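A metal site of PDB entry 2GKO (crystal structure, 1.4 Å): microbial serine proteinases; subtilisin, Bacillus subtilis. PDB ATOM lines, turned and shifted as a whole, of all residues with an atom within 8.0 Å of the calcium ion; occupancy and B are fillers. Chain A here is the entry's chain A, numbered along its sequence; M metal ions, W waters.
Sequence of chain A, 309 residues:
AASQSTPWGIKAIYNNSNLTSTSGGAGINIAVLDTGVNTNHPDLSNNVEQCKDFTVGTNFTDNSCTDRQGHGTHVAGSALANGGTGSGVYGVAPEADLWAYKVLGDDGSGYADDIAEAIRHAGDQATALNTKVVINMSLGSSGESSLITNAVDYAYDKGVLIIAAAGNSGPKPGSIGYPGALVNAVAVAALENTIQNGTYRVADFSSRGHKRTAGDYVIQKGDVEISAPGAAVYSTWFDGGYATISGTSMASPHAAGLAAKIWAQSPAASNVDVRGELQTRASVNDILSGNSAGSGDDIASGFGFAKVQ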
ATOM      1  N   HIS A 210     -12.901 -23.594  22.998  1.00  0.00           N
ATOM      2  CA  HIS A 210     -13.059 -24.397  24.211  1.00  0.00           C
ATOM      3  C   HIS A 210     -11.797 -24.415  25.051  1.00  0.00           C
ATOM      4  O   HIS A 210     -10.686 -24.516  24.507  1.00  0.00           O
ATOM      5  CB  HIS A 210     -13.481 -25.819  23.836  1.00  0.00           C
ATOM      6  CG  HIS A 210     -14.828 -25.897  23.205  1.00  0.00           C
ATOM      7  ND1 HIS A 210     -15.986 -26.035  23.935  1.00  0.00           N
ATOM      8  CD2 HIS A 210     -15.223 -25.777  21.912  1.00  0.00           C
ATOM      9  CE1 HIS A 210     -17.032 -26.011  23.124  1.00  0.00           C
ATOM     10  NE2 HIS A 210     -16.592 -25.842  21.883  1.00  0.00           N
ATOM     11  N   LYS A 211     -11.950 -24.313  26.359  1.00  0.00           N
ATOM     12  CA  LYS A 211     -10.769 -24.190  27.238  1.00  0.00           C
ATOM     13  C   LYS A 211      -9.886 -25.448  27.212  1.00  0.00           C
ATOM     14  O   LYS A 211      -8.664 -25.337  27.301  1.00  0.00           O
ATOM     15  CB  LYS A 211     -11.167 -23.929  28.684  1.00  0.00           C
ATOM     16  CG  LYS A 211     -11.947 -22.673  28.950  1.00  0.00           C
ATOM     17  CD  LYS A 211     -11.991 -22.339  30.420  1.00  0.00           C
ATOM     18  CE  LYS A 211     -12.879 -21.129  30.644  1.00  0.00           C
ATOM     19  NZ  LYS A 211     -13.048 -20.751  32.065  1.00  0.00           N
ATOM     20  N   ARG A 212     -10.476 -26.626  27.095  1.00  0.00           N
ATOM     21  CA  ARG A 212      -9.690 -27.847  27.293  1.00  0.00           C
ATOM     22  C   ARG A 212      -8.718 -28.149  26.155  1.00  0.00           C
ATOM     23  O   ARG A 212      -7.831 -28.990  26.330  1.00  0.00           O
ATOM     24  CB  ARG A 212     -10.569 -29.075  27.592  1.00  0.00           C
ATOM     25  CG  ARG A 212     -11.483 -29.506  26.509  1.00  0.00           C
ATOM     26  CD  ARG A 212     -12.387 -30.629  26.931  1.00  0.00           C
ATOM     27  NE  ARG A 212     -13.436 -30.179  27.838  1.00  0.00           N
ATOM     28  CZ  ARG A 212     -14.206 -30.991  28.548  1.00  0.00           C
ATOM     29  NH1 ARG A 212     -15.149 -30.504  29.336  1.00  0.00           N
ATOM     30  NH2 ARG A 212     -14.049 -32.305  28.477  1.00  0.00           N
ATOM     31  N   THR A 213      -8.881 -27.515  24.997  1.00  0.00           N
ATOM     32  CA  THR A 213      -7.979 -27.767  23.865  1.00  0.00           C
ATOM     33  C   THR A 213      -7.159 -26.557  23.480  1.00  0.00           C
ATOM     34  O   THR A 213      -6.448 -26.589  22.494  1.00  0.00           O
ATOM     35  CB  THR A 213      -8.751 -28.265  22.640  1.00  0.00           C
ATOM     36  OG1 THR A 213      -9.779 -27.330  22.297  1.00  0.00           O
ATOM     37  CG2 THR A 213      -9.479 -29.559  22.908  1.00  0.00           C
ATOM     38  N   ALA A 214      -7.231 -25.503  24.279  1.00  0.00           N
ATOM     39  CA  ALA A 214      -6.551 -24.245  23.975  1.00  0.00           C
ATOM     40  C   ALA A 214      -5.125 -24.225  24.539  1.00  0.00           C
ATOM     41  O   ALA A 214      -4.798 -25.021  25.412  1.00  0.00           O
ATOM     42  CB  ALA A 214      -7.352 -23.076  24.517  1.00  0.00           C
ATOM     43  N   GLY A 215      -4.295 -23.335  24.029  1.00  0.00           N
ATOM     44  CA  GLY A 215      -2.982 -23.068  24.595  1.00  0.00           C
ATOM     45  C   GLY A 215      -1.873 -23.959  24.083  1.00  0.00           C
ATOM     46  O   GLY A 215      -0.766 -23.883  24.593  1.00  0.00           O
ATOM     47  N   ASP A 216      -2.147 -24.795  23.085  1.00  0.00           N
ATOM     48  CA  ASP A 216      -1.152 -25.765  22.600  1.00  0.00           C
ATOM     49  C   ASP A 216      -0.584 -25.457  21.206  1.00  0.00           C
ATOM     50  O   ASP A 216       0.334 -26.159  20.727  1.00  0.00           O
ATOM     51  CB  ASP A 216      -1.694 -27.184  22.676  1.00  0.00           C
ATOM     52  CG  ASP A 216      -2.921 -27.407  21.839  1.00  0.00           C
ATOM     53  OD1 ASP A 216      -3.478 -26.410  21.347  1.00  0.00           O
ATOM     54  OD2 ASP A 216      -3.422 -28.533  21.621  1.00  0.00           O
ATOM     55  N   TYR A 217      -1.089 -24.409  20.561  1.00  0.00           N
ATOM     56  CA  TYR A 217      -0.689 -24.051  19.205  1.00  0.00           C
ATOM     57  C   TYR A 217      -0.846 -25.228  18.241  1.00  0.00           C
ATOM     58  O   TYR A 217      -0.052 -25.403  17.305  1.00  0.00           O
ATOM     59  CB  TYR A 217       0.733 -23.484  19.192  1.00  0.00           C
ATOM     60  CG  TYR A 217       0.858 -22.066  19.704  1.00  0.00           C
ATOM     61  CD1 TYR A 217       1.355 -21.815  20.994  1.00  0.00           C
ATOM     62  CD2 TYR A 217       0.530 -20.967  18.915  1.00  0.00           C
ATOM     63  CE1 TYR A 217       1.508 -20.535  21.460  1.00  0.00           C
ATOM     64  CE2 TYR A 217       0.679 -19.677  19.382  1.00  0.00           C
ATOM     65  CZ  TYR A 217       1.167 -19.462  20.670  1.00  0.00           C
ATOM     66  OH  TYR A 217       1.348 -18.183  21.169  1.00  0.00           O
ATOM     67  N   VAL A 218      -1.889 -26.024  18.466  1.00  0.00           N
ATOM     68  CA  VAL A 218      -2.260 -27.125  17.598  1.00  0.00           C
ATOM     69  C   VAL A 218      -3.772 -27.108  17.471  1.00  0.00           C
ATOM     70  O   VAL A 218      -4.473 -27.115  18.486  1.00  0.00           O
ATOM     71  CB  VAL A 218      -1.817 -28.487  18.192  1.00  0.00           C
ATOM     72  CG1 VAL A 218      -2.368 -29.637  17.387  1.00  0.00           C
ATOM     73  CG2 VAL A 218      -0.293 -28.562  18.287  1.00  0.00           C
ATOM     74  N   ILE A 219      -4.292 -27.083  16.252  1.00  0.00           N
ATOM     75  CA  ILE A 219      -5.730 -26.947  16.057  1.00  0.00           C
ATOM     76  C   ILE A 219      -6.445 -28.285  16.123  1.00  0.00           C
ATOM     77  O   ILE A 219      -6.180 -29.192  15.338  1.00  0.00           O
ATOM     78  CB  ILE A 219      -6.041 -26.252  14.708  1.00  0.00           C
ATOM     79  CG1 ILE A 219      -5.419 -24.861  14.657  1.00  0.00           C
ATOM     80  CG2 ILE A 219      -7.565 -26.278  14.407  1.00  0.00           C
ATOM     81  CD1 ILE A 219      -5.994 -23.837  15.632  1.00  0.00           C
ATOM     82  N   GLN A 220      -7.380 -28.366  17.075  1.00  0.00           N
ATOM     83  CA  GLN A 220      -8.350 -29.440  17.152  1.00  0.00           C
ATOM     84  C   GLN A 220      -9.718 -28.868  16.853  1.00  0.00           C
ATOM     85  O   GLN A 220      -9.897 -27.653  16.826  1.00  0.00           O
ATOM     86  CB  GLN A 220      -8.358 -30.051  18.568  1.00  0.00           C
ATOM     87  CG  GLN A 220      -7.054 -30.750  18.966  1.00  0.00           C
ATOM     88  CD  GLN A 220      -6.037 -29.867  19.668  1.00  0.00           C
ATOM     89  OE1 GLN A 220      -6.363 -28.838  20.242  1.00  0.00           O
ATOM     90  NE2 GLN A 220      -4.770 -30.286  19.644  1.00  0.00           N
ATOM     91  N   LYS A 221     -10.673 -29.762  16.618  1.00  0.00           N
ATOM     92  CA  LYS A 221     -12.082 -29.398  16.547  1.00  0.00           C
ATOM     93  C   LYS A 221     -12.431 -28.527  17.755  1.00  0.00           C
ATOM     94  O   LYS A 221     -12.123 -28.893  18.909  1.00  0.00           O
ATOM     95  CB  LYS A 221     -12.949 -30.657  16.503  1.00  0.00           C
ATOM     96  CG  LYS A 221     -14.422 -30.425  16.239  1.00  0.00           C
ATOM     97  CD  LYS A 221     -15.179 -31.730  16.092  1.00  0.00           C
ATOM     98  CE  LYS A 221     -16.636 -31.480  15.719  1.00  0.00           C
ATOM     99  NZ  LYS A 221     -17.440 -32.757  15.519  1.00  0.00           N
ATOM    100  N   GLY A 222     -13.052 -27.377  17.507  1.00  0.00           N
ATOM    101  CA  GLY A 222     -13.462 -26.471  18.581  1.00  0.00           C
ATOM    102  C   GLY A 222     -12.525 -25.322  18.907  1.00  0.00           C
ATOM    103  O   GLY A 222     -12.823 -24.501  19.765  1.00  0.00           O
ATOM    104  N   ASP A 223     -11.408 -25.228  18.202  1.00  0.00           N
ATOM    105  CA  ASP A 223     -10.434 -24.159  18.416  1.00  0.00           C
ATOM    106  C   ASP A 223     -10.607 -22.997  17.453  1.00  0.00           C
ATOM    107  O   ASP A 223     -10.768 -23.202  16.244  1.00  0.00           O
ATOM    108  CB  ASP A 223      -9.003 -24.669  18.211  1.00  0.00           C
ATOM    109  CG  ASP A 223      -8.573 -25.613  19.277  1.00  0.00           C
ATOM    110  OD1 ASP A 223      -7.536 -26.302  19.050  1.00  0.00           O
ATOM    111  OD2 ASP A 223      -9.192 -25.732  20.354  1.00  0.00           O
ATOM    112  N   VAL A 224     -10.566 -21.785  17.988  1.00  0.00           N
ATOM    113  CA  VAL A 224     -10.341 -20.571  17.211  1.00  0.00           C
ATOM    114  C   VAL A 224      -8.877 -20.611  16.740  1.00  0.00           C
ATOM    115  O   VAL A 224      -8.009 -21.070  17.455  1.00  0.00           O
ATOM    116  CB  VAL A 224     -10.604 -19.296  18.044  1.00  0.00           C
ATOM    117  CG1 VAL A 224     -10.160 -18.053  17.308  1.00  0.00           C
ATOM    118  CG2 VAL A 224     -12.119 -19.207  18.453  1.00  0.00           C
ATOM    119  N   ASP A 297      -1.618 -18.928  22.831  1.00  0.00           N
ATOM    120  CA  ASP A 297      -2.753 -19.428  22.078  1.00  0.00           C
ATOM    121  C   ASP A 297      -3.963 -19.442  23.030  1.00  0.00           C
ATOM    122  O   ASP A 297      -3.931 -20.146  24.033  1.00  0.00           O
ATOM    123  CB  ASP A 297      -2.402 -20.818  21.578  1.00  0.00           C
ATOM    124  CG  ASP A 297      -3.562 -21.550  20.972  1.00  0.00           C
ATOM    125  OD1 ASP A 297      -3.489 -22.788  20.959  1.00  0.00           O
ATOM    126  OD2 ASP A 297      -4.580 -20.967  20.513  1.00  0.00           O
ATOM    127  N   PHE A 303      -4.173 -18.252  17.714  1.00  0.00           N
ATOM    128  CA  PHE A 303      -2.716 -18.064  17.736  1.00  0.00           C
ATOM    129  C   PHE A 303      -2.319 -16.598  17.690  1.00  0.00           C
ATOM    130  O   PHE A 303      -1.205 -16.224  18.114  1.00  0.00           O
ATOM    131  CB  PHE A 303      -2.053 -18.770  16.552  1.00  0.00           C
ATOM    132  CG  PHE A 303      -2.206 -20.281  16.517  1.00  0.00           C
ATOM    133  CD1 PHE A 303      -3.016 -20.994  17.418  1.00  0.00           C
ATOM    134  CD2 PHE A 303      -1.510 -20.992  15.546  1.00  0.00           C
ATOM    135  CE1 PHE A 303      -3.151 -22.350  17.331  1.00  0.00           C
ATOM    136  CE2 PHE A 303      -1.635 -22.345  15.460  1.00  0.00           C
ATOM    137  CZ  PHE A 303      -2.438 -23.045  16.353  1.00  0.00           C
HETATM  138 CA    CA M   1      -5.663 -26.669  20.386  1.00  0.00          CA
HETATM  139  O   HOH W   1      -5.484 -24.280  20.075  1.00  0.00           O
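Within 4 Å of the calcium ion: Thr 213, Asp 216, Val 218, Gln 220 and Asp 223.
The nearest printed residue that does not touch the calcium ion is Ile 219 (4.3 Å).
OD1 of Asp 297 sits at hydrogen-bond distance from N of Asp 216 (3.2 Å).
The calcium ion is bound by O of Thr 213, OE1 of Gln 220, O of Val 218, OD1 of Asp 223, OD1 of Asp 216 and water W1.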
